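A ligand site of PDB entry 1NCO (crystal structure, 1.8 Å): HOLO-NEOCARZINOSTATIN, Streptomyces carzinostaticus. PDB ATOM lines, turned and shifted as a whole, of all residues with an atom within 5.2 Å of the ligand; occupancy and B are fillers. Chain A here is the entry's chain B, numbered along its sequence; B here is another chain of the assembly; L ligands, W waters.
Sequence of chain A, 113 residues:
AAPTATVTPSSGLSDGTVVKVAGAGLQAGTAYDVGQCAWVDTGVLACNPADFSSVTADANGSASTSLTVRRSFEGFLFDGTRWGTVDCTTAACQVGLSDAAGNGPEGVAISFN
An oxygen (O8) of the ligand sits at hydrogen-bond distance from the backbone NH (N) of Ala 1 of chain B (2.6 Å).
The side-chain hydroxyl of Ser 98 sits at hydrogen-bond distance from an oxygen (O7) of the ligand, at 3.1 Å.
N of Gly 35 lies within hydrogen-bond range of O9 of the ligand, 3.1 Å away.
N of Gly 80 sits at hydrogen-bond distance from O12 of the ligand, at 3.4 Å.
N of Ala 1 of chain B is in hydrogen-bond range of O of Gly 102.
N of Cys 47 lies within hydrogen-bond range of O of Phe 76, at 2.8 Å.
The backbone carbonyl oxygen of Ser 98 sits at hydrogen-bond distance from the backbone NH of Asp 33, at 2.8 Å.
The backbone NH of Gly 35 sits at hydrogen-bond distance from the backbone carbonyl oxygen of Gly 96 (2.9 Å).
The side-chain carboxylate of Asp 99 is in hydrogen-bond range of the backbone NH of Gly 102 (3.2 Å).
SG of Cys 47 is disulfide-bonded to SG of Cys 37 (2.0 Å).
N of Gln 94 is in hydrogen-bond range of O of Cys 37, 2.8 Å away.
N of Ala 101 sits at hydrogen-bond distance from OD1 of Asp 99 (3.0 Å).
O of Leu 77 sits close to O12 of the ligand (3.5 Å).
O of Phe 78 sits close to O12 of the ligand, at 3.4 Å.
An oxygen (O7) of the ligand lies close to the backbone carbonyl oxygen (O) of Gly 102 (3.2 Å).
Residues that only touch the ligand: Phe 76 (3.0 Å), Pro 49 (3.3 Å), Cys 47 (3.3 Å), Cys 37 (3.4 Å), Gly 96 (3.4 Å), Phe 52 (3.5 Å), Trp 39 (3.5 Å), Leu 45 (3.6 Å), Ala 100 (3.6 Å), Gln 94 (3.6 Å), Val 95 (3.7 Å), Ala 101 (3.7 Å), Gly 43 (3.8 Å) and Val 34 (3.9 Å).
Within 4 Å of the ligand: Val 34, Gly 35, Cys 37, Trp 39, Gly 43, Leu 45, Cys 47, Pro 49, Phe 52, Phe 76, Leu 77, Phe 78, Gly 80, Gln 94, Val 95, Gly 96, Ser 98, Ala 100, Ala 101, Gly 102 and Ala 1 of chain B.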
ATOM      1  N   ASP A  33      24.857  38.298 -11.010  1.00  0.00           N
ATOM      2  CA  ASP A  33      24.963  38.007  -9.593  1.00  0.00           C
ATOM      3  C   ASP A  33      26.442  37.749  -9.283  1.00  0.00           C
ATOM      4  O   ASP A  33      27.259  37.449 -10.172  1.00  0.00           O
ATOM      5  CB  ASP A  33      24.092  36.808  -9.250  1.00  0.00           C
ATOM      6  CG  ASP A  33      22.645  37.222  -8.975  1.00  0.00           C
ATOM      7  OD1 ASP A  33      22.395  38.195  -8.305  1.00  0.00           O
ATOM      8  OD2 ASP A  33      21.737  36.580  -9.414  1.00  0.00           O
ATOM      9  N   VAL A  34      26.788  38.014  -8.033  1.00  0.00           N
ATOM     10  CA  VAL A  34      28.174  37.908  -7.583  1.00  0.00           C
ATOM     11  C   VAL A  34      28.158  36.984  -6.377  1.00  0.00           C
ATOM     12  O   VAL A  34      27.445  37.293  -5.420  1.00  0.00           O
ATOM     13  CB  VAL A  34      28.712  39.336  -7.194  1.00  0.00           C
ATOM     14  CG1 VAL A  34      30.091  39.176  -6.563  1.00  0.00           C
ATOM     15  CG2 VAL A  34      28.893  40.251  -8.395  1.00  0.00           C
ATOM     16  N   GLY A  35      28.907  35.903  -6.287  1.00  0.00           N
ATOM     17  CA  GLY A  35      28.821  35.071  -5.100  1.00  0.00           C
ATOM     18  C   GLY A  35      29.958  34.097  -4.956  1.00  0.00           C
ATOM     19  O   GLY A  35      30.922  34.096  -5.725  1.00  0.00           O
ATOM     20  N   GLN A  36      29.852  33.316  -3.905  1.00  0.00           N
ATOM     21  CA  GLN A  36      30.833  32.290  -3.579  1.00  0.00           C
ATOM     22  C   GLN A  36      30.239  30.912  -3.788  1.00  0.00           C
ATOM     23  O   GLN A  36      29.175  30.562  -3.258  1.00  0.00           O
ATOM     24  CB  GLN A  36      31.242  32.494  -2.135  1.00  0.00           C
ATOM     25  CG  GLN A  36      32.263  31.531  -1.566  1.00  0.00           C
ATOM     26  CD  GLN A  36      32.406  31.637  -0.061  1.00  0.00           C
ATOM     27  OE1 GLN A  36      31.874  32.533   0.610  1.00  0.00           O
ATOM     28  NE2 GLN A  36      33.146  30.693   0.516  1.00  0.00           N
ATOM     29  N   CYS A  37      30.937  30.124  -4.578  1.00  0.00           N
ATOM     30  CA  CYS A  37      30.552  28.796  -4.930  1.00  0.00           C
ATOM     31  C   CYS A  37      31.753  27.849  -4.871  1.00  0.00           C
ATOM     32  O   CYS A  37      32.900  28.290  -4.657  1.00  0.00           O
ATOM     33  CB  CYS A  37      29.958  28.788  -6.340  1.00  0.00           C
ATOM     34  SG  CYS A  37      28.594  29.926  -6.677  1.00  0.00           S
ATOM     35  N   TRP A  39      32.807  23.825  -6.942  1.00  0.00           N
ATOM     36  CA  TRP A  39      32.366  22.703  -7.725  1.00  0.00           C
ATOM     37  C   TRP A  39      32.503  21.508  -6.803  1.00  0.00           C
ATOM     38  O   TRP A  39      33.580  21.244  -6.271  1.00  0.00           O
ATOM     39  CB  TRP A  39      33.208  22.517  -8.961  1.00  0.00           C
ATOM     40  CG  TRP A  39      32.405  22.934 -10.169  1.00  0.00           C
ATOM     41  CD1 TRP A  39      31.380  22.211 -10.782  1.00  0.00           C
ATOM     42  CD2 TRP A  39      32.611  24.095 -10.792  1.00  0.00           C
ATOM     43  NE1 TRP A  39      30.939  22.938 -11.796  1.00  0.00           N
ATOM     44  CE2 TRP A  39      31.665  24.070 -11.815  1.00  0.00           C
ATOM     45  CE3 TRP A  39      33.474  25.101 -10.545  1.00  0.00           C
ATOM     46  CZ2 TRP A  39      31.566  25.107 -12.674  1.00  0.00           C
ATOM     47  CZ3 TRP A  39      33.364  26.144 -11.430  1.00  0.00           C
ATOM     48  CH2 TRP A  39      32.432  26.147 -12.460  1.00  0.00           C
ATOM     49  N   GLY A  43      30.252  18.895 -13.079  1.00  0.00           N
ATOM     50  CA  GLY A  43      29.171  19.771 -13.484  1.00  0.00           C
ATOM     51  C   GLY A  43      28.309  20.227 -12.301  1.00  0.00           C
ATOM     52  O   GLY A  43      27.261  20.814 -12.585  1.00  0.00           O
ATOM     53  N   VAL A  44      28.586  20.075 -11.012  1.00  0.00           N
ATOM     54  CA  VAL A  44      27.610  20.467  -9.991  1.00  0.00           C
ATOM     55  C   VAL A  44      28.279  21.568  -9.202  1.00  0.00           C
ATOM     56  O   VAL A  44      29.335  21.349  -8.595  1.00  0.00           O
ATOM     57  CB  VAL A  44      27.222  19.232  -9.046  1.00  0.00           C
ATOM     58  CG1 VAL A  44      26.322  19.660  -7.884  1.00  0.00           C
ATOM     59  CG2 VAL A  44      26.347  18.205  -9.783  1.00  0.00           C
ATOM     60  N   LEU A  45      27.676  22.750  -9.236  1.00  0.00           N
ATOM     61  CA  LEU A  45      28.183  23.905  -8.505  1.00  0.00           C
ATOM     62  C   LEU A  45      27.238  24.256  -7.366  1.00  0.00           C
ATOM     63  O   LEU A  45      26.054  24.525  -7.597  1.00  0.00           O
ATOM     64  CB  LEU A  45      28.280  25.092  -9.485  1.00  0.00           C
ATOM     65  CG  LEU A  45      28.873  26.408  -9.029  1.00  0.00           C
ATOM     66  CD1 LEU A  45      30.379  26.238  -8.883  1.00  0.00           C
ATOM     67  CD2 LEU A  45      28.542  27.510 -10.024  1.00  0.00           C
ATOM     68  N   ALA A  46      27.761  24.316  -6.141  1.00  0.00           N
ATOM     69  CA  ALA A  46      26.982  24.624  -4.974  1.00  0.00           C
ATOM     70  C   ALA A  46      27.472  25.982  -4.567  1.00  0.00           C
ATOM     71  O   ALA A  46      28.678  26.260  -4.600  1.00  0.00           O
ATOM     72  CB  ALA A  46      27.248  23.631  -3.837  1.00  0.00           C
ATOM     73  N   CYS A  47      26.531  26.853  -4.204  1.00  0.00           N
ATOM     74  CA  CYS A  47      26.832  28.234  -3.873  1.00  0.00           C
ATOM     75  C   CYS A  47      26.285  28.643  -2.515  1.00  0.00           C
ATOM     76  O   CYS A  47      25.576  27.870  -1.831  1.00  0.00           O
ATOM     77  CB  CYS A  47      26.242  29.149  -4.927  1.00  0.00           C
ATOM     78  SG  CYS A  47      26.873  28.872  -6.591  1.00  0.00           S
ATOM     79  N   ASN A  48      26.656  29.853  -2.099  1.00  0.00           N
ATOM     80  CA  ASN A  48      26.178  30.396  -0.872  1.00  0.00           C
ATOM     81  C   ASN A  48      25.231  31.557  -1.172  1.00  0.00           C
ATOM     82  O   ASN A  48      25.601  32.716  -0.934  1.00  0.00           O
ATOM     83  CB  ASN A  48      27.382  30.834  -0.067  1.00  0.00           C
ATOM     84  CG  ASN A  48      27.026  31.496   1.238  1.00  0.00           C
ATOM     85  OD1 ASN A  48      27.628  32.495   1.597  1.00  0.00           O
ATOM     86  ND2 ASN A  48      26.065  31.045   2.031  1.00  0.00           N
ATOM     87  N   PRO A  49      24.002  31.373  -1.691  1.00  0.00           N
ATOM     88  CA  PRO A  49      23.114  32.464  -2.073  1.00  0.00           C
ATOM     89  C   PRO A  49      22.787  33.489  -1.009  1.00  0.00           C
ATOM     90  O   PRO A  49      22.611  34.653  -1.361  1.00  0.00           O
ATOM     91  CB  PRO A  49      21.893  31.778  -2.639  1.00  0.00           C
ATOM     92  CG  PRO A  49      21.851  30.463  -1.920  1.00  0.00           C
ATOM     93  CD  PRO A  49      23.315  30.088  -1.821  1.00  0.00           C
ATOM     94  N   PHE A  52      25.026  36.529  -1.598  1.00  0.00           N
ATOM     95  CA  PHE A  52      25.253  37.032  -2.943  1.00  0.00           C
ATOM     96  C   PHE A  52      25.068  38.534  -3.051  1.00  0.00           C
ATOM     97  O   PHE A  52      24.342  39.140  -2.262  1.00  0.00           O
ATOM     98  CB  PHE A  52      24.304  36.406  -3.937  1.00  0.00           C
ATOM     99  CG  PHE A  52      24.599  34.998  -4.464  1.00  0.00           C
ATOM    100  CD1 PHE A  52      25.557  34.167  -3.923  1.00  0.00           C
ATOM    101  CD2 PHE A  52      23.838  34.531  -5.517  1.00  0.00           C
ATOM    102  CE1 PHE A  52      25.745  32.906  -4.430  1.00  0.00           C
ATOM    103  CE2 PHE A  52      24.025  33.269  -6.025  1.00  0.00           C
ATOM    104  CZ  PHE A  52      24.988  32.448  -5.483  1.00  0.00           C
ATOM    105  N   PHE A  76      24.022  25.378  -1.955  1.00  0.00           N
ATOM    106  CA  PHE A  76      22.770  25.208  -2.674  1.00  0.00           C
ATOM    107  C   PHE A  76      23.058  25.143  -4.159  1.00  0.00           C
ATOM    108  O   PHE A  76      24.027  25.767  -4.598  1.00  0.00           O
ATOM    109  CB  PHE A  76      21.793  26.369  -2.422  1.00  0.00           C
ATOM    110  CG  PHE A  76      21.154  26.298  -1.061  1.00  0.00           C
ATOM    111  CD1 PHE A  76      21.785  26.897   0.026  1.00  0.00           C
ATOM    112  CD2 PHE A  76      19.942  25.627  -0.915  1.00  0.00           C
ATOM    113  CE1 PHE A  76      21.218  26.808   1.264  1.00  0.00           C
ATOM    114  CE2 PHE A  76      19.388  25.554   0.338  1.00  0.00           C
ATOM    115  CZ  PHE A  76      20.027  26.140   1.418  1.00  0.00           C
ATOM    116  N   LEU A  77      22.261  24.352  -4.881  1.00  0.00           N
ATOM    117  CA  LEU A  77      22.345  24.132  -6.291  1.00  0.00           C
ATOM    118  C   LEU A  77      21.482  25.115  -7.051  1.00  0.00           C
ATOM    119  O   LEU A  77      20.633  25.795  -6.467  1.00  0.00           O
ATOM    120  CB  LEU A  77      21.903  22.744  -6.554  1.00  0.00           C
ATOM    121  CG  LEU A  77      22.947  21.654  -6.658  1.00  0.00           C
ATOM    122  CD1 LEU A  77      24.156  21.936  -5.791  1.00  0.00           C
ATOM    123  CD2 LEU A  77      22.228  20.357  -6.343  1.00  0.00           C
ATOM    124  N   PHE A  78      21.637  25.246  -8.360  1.00  0.00           N
ATOM    125  CA  PHE A  78      20.871  26.227  -9.138  1.00  0.00           C
ATOM    126  C   PHE A  78      19.340  26.074  -9.012  1.00  0.00           C
ATOM    127  O   PHE A  78      18.602  27.068  -9.009  1.00  0.00           O
ATOM    128  CB  PHE A  78      21.322  26.130 -10.609  1.00  0.00           C
ATOM    129  CG  PHE A  78      20.756  27.254 -11.432  1.00  0.00           C
ATOM    130  CD1 PHE A  78      21.126  28.560 -11.158  1.00  0.00           C
ATOM    131  CD2 PHE A  78      19.863  26.985 -12.467  1.00  0.00           C
ATOM    132  CE1 PHE A  78      20.617  29.614 -11.905  1.00  0.00           C
ATOM    133  CE2 PHE A  78      19.373  28.053 -13.219  1.00  0.00           C
ATOM    134  CZ  PHE A  78      19.740  29.350 -12.946  1.00  0.00           C
ATOM    135  N   ASP A  79      18.807  24.884  -8.775  1.00  0.00           N
ATOM    136  CA  ASP A  79      17.384  24.712  -8.653  1.00  0.00           C
ATOM    137  C   ASP A  79      16.816  25.009  -7.265  1.00  0.00           C
ATOM    138  O   ASP A  79      15.724  24.590  -6.952  1.00  0.00           O
ATOM    139  CB  ASP A  79      17.085  23.291  -9.034  1.00  0.00           C
ATOM    140  CG  ASP A  79      17.799  22.227  -8.173  1.00  0.00           C
ATOM    141  OD1 ASP A  79      18.471  22.572  -7.197  1.00  0.00           O
ATOM    142  OD2 ASP A  79      17.671  21.045  -8.475  1.00  0.00           O
ATOM    143  N   GLY A  80      17.580  25.626  -6.366  1.00  0.00           N
ATOM    144  CA  GLY A  80      17.114  25.943  -5.049  1.00  0.00           C
ATOM    145  C   GLY A  80      17.289  24.795  -4.084  1.00  0.00           C
ATOM    146  O   GLY A  80      16.987  24.997  -2.907  1.00  0.00           O
ATOM    147  N   THR A  81      17.723  23.570  -4.477  1.00  0.00           N
ATOM    148  CA  THR A  81      17.914  22.501  -3.500  1.00  0.00           C
ATOM    149  C   THR A  81      19.301  22.562  -2.866  1.00  0.00           C
ATOM    150  O   THR A  81      20.242  23.152  -3.419  1.00  0.00           O
ATOM    151  CB  THR A  81      17.706  21.130  -4.137  1.00  0.00           C
ATOM    152  OG1 THR A  81      18.660  20.947  -5.144  1.00  0.00           O
ATOM    153  CG2 THR A  81      16.385  21.027  -4.841  1.00  0.00           C
ATOM    154  N   GLN A  94      35.470  29.502  -4.680  1.00  0.00           N
ATOM    155  CA  GLN A  94      35.751  30.543  -5.642  1.00  0.00           C
ATOM    156  C   GLN A  94      34.712  31.628  -5.493  1.00  0.00           C
ATOM    157  O   GLN A  94      33.639  31.387  -4.939  1.00  0.00           O
ATOM    158  CB  GLN A  94      35.618  30.006  -7.026  1.00  0.00           C
ATOM    159  CG  GLN A  94      36.713  29.074  -7.471  1.00  0.00           C
ATOM    160  CD  GLN A  94      36.336  28.429  -8.775  1.00  0.00           C
ATOM    161  OE1 GLN A  94      35.726  29.079  -9.632  1.00  0.00           O
ATOM    162  NE2 GLN A  94      36.735  27.195  -9.020  1.00  0.00           N
ATOM    163  N   VAL A  95      35.028  32.832  -5.963  1.00  0.00           N
ATOM    164  CA  VAL A  95      34.114  33.951  -5.900  1.00  0.00           C
ATOM    165  C   VAL A  95      34.076  34.422  -7.335  1.00  0.00           C
ATOM    166  O   VAL A  95      35.092  34.500  -8.005  1.00  0.00           O
ATOM    167  CB  VAL A  95      34.640  35.005  -4.925  1.00  0.00           C
ATOM    168  CG1 VAL A  95      33.977  36.385  -5.138  1.00  0.00           C
ATOM    169  CG2 VAL A  95      34.335  34.493  -3.501  1.00  0.00           C
ATOM    170  N   GLY A  96      32.872  34.636  -7.855  1.00  0.00           N
ATOM    171  CA  GLY A  96      32.764  35.074  -9.227  1.00  0.00           C
ATOM    172  C   GLY A  96      31.453  35.790  -9.492  1.00  0.00           C
ATOM    173  O   GLY A  96      30.693  36.154  -8.597  1.00  0.00           O
ATOM    174  N   LEU A  97      31.239  36.002 -10.762  1.00  0.00           N
ATOM    175  CA  LEU A  97      30.102  36.746 -11.254  1.00  0.00           C
ATOM    176  C   LEU A  97      29.436  35.900 -12.299  1.00  0.00           C
ATOM    177  O   LEU A  97      30.143  35.201 -13.047  1.00  0.00           O
ATOM    178  CB  LEU A  97      30.513  38.090 -11.922  1.00  0.00           C
ATOM    179  CG  LEU A  97      31.336  39.134 -11.151  1.00  0.00           C
ATOM    180  CD1 LEU A  97      32.822  38.870 -11.336  1.00  0.00           C
ATOM    181  CD2 LEU A  97      31.053  40.504 -11.698  1.00  0.00           C
ATOM    182  N   SER A  98      28.108  35.998 -12.390  1.00  0.00           N
ATOM    183  CA  SER A  98      27.340  35.171 -13.322  1.00  0.00           C
ATOM    184  C   SER A  98      26.060  35.848 -13.776  1.00  0.00           C
ATOM    185  O   SER A  98      25.348  36.358 -12.914  1.00  0.00           O
ATOM    186  CB  SER A  98      26.989  33.878 -12.637  1.00  0.00           C
ATOM    187  OG  SER A  98      26.478  32.989 -13.594  1.00  0.00           O
ATOM    188  N   ASP A  99      25.743  35.875 -15.062  1.00  0.00           N
ATOM    189  CA  ASP A  99      24.485  36.441 -15.576  1.00  0.00           C
ATOM    190  C   ASP A  99      23.414  35.371 -15.510  1.00  0.00           C
ATOM    191  O   ASP A  99      23.692  34.228 -15.103  1.00  0.00           O
ATOM    192  CB  ASP A  99      24.598  36.899 -17.032  1.00  0.00           C
ATOM    193  CG  ASP A  99      24.988  35.908 -18.140  1.00  0.00           C
ATOM    194  OD1 ASP A  99      24.863  34.713 -17.996  1.00  0.00           O
ATOM    195  OD2 ASP A  99      25.413  36.314 -19.199  1.00  0.00           O
ATOM    196  N   ALA A 100      22.205  35.617 -16.012  1.00  0.00           N
ATOM    197  CA  ALA A 100      21.164  34.626 -15.876  1.00  0.00           C
ATOM    198  C   ALA A 100      21.464  33.319 -16.618  1.00  0.00           C
ATOM    199  O   ALA A 100      20.998  32.291 -16.165  1.00  0.00           O
ATOM    200  CB  ALA A 100      19.861  35.208 -16.375  1.00  0.00           C
ATOM    201  N   ALA A 101      22.274  33.258 -17.659  1.00  0.00           N
ATOM    202  CA  ALA A 101      22.610  32.020 -18.360  1.00  0.00           C
ATOM    203  C   ALA A 101      23.823  31.272 -17.767  1.00  0.00           C
ATOM    204  O   ALA A 101      24.169  30.183 -18.239  1.00  0.00           O
ATOM    205  CB  ALA A 101      22.932  32.344 -19.790  1.00  0.00           C
ATOM    206  N   GLY A 102      24.468  31.773 -16.734  1.00  0.00           N
ATOM    207  CA  GLY A 102      25.640  31.116 -16.149  1.00  0.00           C
ATOM    208  C   GLY A 102      26.966  31.699 -16.675  1.00  0.00           C
ATOM    209  O   GLY A 102      28.067  31.269 -16.328  1.00  0.00           O
ATOM    210  N   ASN A 103      26.873  32.779 -17.439  1.00  0.00           N
ATOM    211  CA  ASN A 103      28.037  33.306 -18.113  1.00  0.00           C
ATOM    212  C   ASN A 103      28.647  34.465 -17.379  1.00  0.00           C
ATOM    213  O   ASN A 103      27.985  35.283 -16.717  1.00  0.00           O
ATOM    214  CB  ASN A 103      27.703  33.780 -19.544  1.00  0.00           C
ATOM    215  CG  ASN A 103      27.339  32.698 -20.525  1.00  0.00           C
ATOM    216  OD1 ASN A 103      27.516  31.481 -20.329  1.00  0.00           O
ATOM    217  ND2 ASN A 103      26.753  33.101 -21.626  1.00  0.00           N
ATOM    218  N   GLY A 107      35.739  31.952 -12.323  1.00  0.00           N
ATOM    219  CA  GLY A 107      35.747  32.137 -10.890  1.00  0.00           C
ATOM    220  C   GLY A 107      37.183  32.362 -10.396  1.00  0.00           C
ATOM    221  O   GLY A 107      38.146  31.922 -11.027  1.00  0.00           O
ATOM    222  N   ALA B   1      30.428  30.412 -16.012  1.00  0.00           N
ATOM    223  CA  ALA B   1      30.817  29.561 -17.116  1.00  0.00           C
ATOM    224  C   ALA B   1      31.649  30.533 -17.916  1.00  0.00           C
ATOM    225  O   ALA B   1      31.049  31.198 -18.749  1.00  0.00           O
ATOM    226  CB  ALA B   1      29.604  29.151 -17.958  1.00  0.00           C
HETATM  227  C1  LIG L   1      23.977  30.064  -9.692  1.00  0.00           C
HETATM  228  C2  LIG L   1      23.181  30.389  -8.679  1.00  0.00           C
HETATM  229  C3  LIG L   1      22.578  30.327  -7.592  1.00  0.00           C
HETATM  230  C4  LIG L   1      22.083  29.848  -6.235  1.00  0.00           C
HETATM  231  O1  LIG L   1      22.998  29.621  -5.125  1.00  0.00           O
HETATM  232  C5  LIG L   1      22.629  28.456  -5.840  1.00  0.00           C
HETATM  233  C6  LIG L   1      23.486  27.783  -6.813  1.00  0.00           C
HETATM  234  C7  LIG L   1      24.119  27.539  -7.821  1.00  0.00           C
HETATM  235  C8  LIG L   1      24.645  27.672  -9.023  1.00  0.00           C
HETATM  236  C9  LIG L   1      24.607  28.735  -9.831  1.00  0.00           C
HETATM  237  C10 LIG L   1      25.199  28.744 -11.259  1.00  0.00           C
HETATM  238  O2  LIG L   1      24.314  27.976 -12.118  1.00  0.00           O
HETATM  239  C11 LIG L   1      25.250  30.233 -11.655  1.00  0.00           C
HETATM  240  O3  LIG L   1      26.586  30.771 -11.381  1.00  0.00           O
HETATM  241  C12 LIG L   1      24.188  30.871 -10.750  1.00  0.00           C
HETATM  242  C13 LIG L   1      24.874  27.696 -13.403  1.00  0.00           C
HETATM  243  O4  LIG L   1      25.962  26.763 -13.268  1.00  0.00           O
HETATM  244  C14 LIG L   1      23.833  27.121 -14.337  1.00  0.00           C
HETATM  245  N1  LIG L   1      22.609  27.864 -14.403  1.00  0.00           N
HETATM  246  C15 LIG L   1      22.558  29.269 -14.862  1.00  0.00           C
HETATM  247  C16 LIG L   1      23.381  25.818 -13.855  1.00  0.00           C
HETATM  248  O5  LIG L   1      22.475  25.389 -14.844  1.00  0.00           O
HETATM  249  C17 LIG L   1      24.562  24.853 -13.760  1.00  0.00           C
HETATM  250  O6  LIG L   1      25.045  24.690 -15.078  1.00  0.00           O
HETATM  251  C18 LIG L   1      25.578  25.477 -12.795  1.00  0.00           C
HETATM  252  C19 LIG L   1      26.849  24.635 -12.781  1.00  0.00           C
HETATM  253  C20 LIG L   1      27.685  30.420 -12.287  1.00  0.00           C
HETATM  254  O7  LIG L   1      27.347  30.035 -13.411  1.00  0.00           O
HETATM  255  C21 LIG L   1      29.084  30.544 -11.960  1.00  0.00           C
HETATM  256  C22 LIG L   1      30.043  29.722 -12.626  1.00  0.00           C
HETATM  257  O8  LIG L   1      29.751  29.082 -13.848  1.00  0.00           O
HETATM  258  C23 LIG L   1      31.307  29.471 -12.062  1.00  0.00           C
HETATM  259  C24 LIG L   1      31.665  30.057 -10.867  1.00  0.00           C
HETATM  260  C25 LIG L   1      30.779  30.917 -10.231  1.00  0.00           C
HETATM  261  C26 LIG L   1      29.505  31.170 -10.766  1.00  0.00           C
HETATM  262  C27 LIG L   1      28.658  32.055 -10.086  1.00  0.00           C
HETATM  263  C28 LIG L   1      29.022  32.661  -8.912  1.00  0.00           C
HETATM  264  O9  LIG L   1      28.187  33.542  -8.237  1.00  0.00           O
HETATM  265  C29 LIG L   1      26.761  33.619  -8.393  1.00  0.00           C
HETATM  266  C30 LIG L   1      30.258  32.382  -8.398  1.00  0.00           C
HETATM  267  C31 LIG L   1      31.136  31.515  -9.047  1.00  0.00           C
HETATM  268  C32 LIG L   1      32.458  31.267  -8.389  1.00  0.00           C
HETATM  269  C33 LIG L   1      20.609  30.210  -5.977  1.00  0.00           C
HETATM  270  O10 LIG L   1      20.246  29.763  -4.693  1.00  0.00           O
HETATM  271  C34 LIG L   1      19.248  28.914  -4.803  1.00  0.00           C
HETATM  272  O11 LIG L   1      18.659  28.418  -3.859  1.00  0.00           O
HETATM  273  O12 LIG L   1      18.861  28.772  -6.051  1.00  0.00           O
HETATM  274  C35 LIG L   1      19.587  29.615  -6.892  1.00  0.00           C
HETATM  275  O   HOH W   1      20.943  23.402 -12.497  1.00  0.00           O
HETATM  276  O   HOH W   2      32.020  33.079 -12.178  1.00  0.00           O
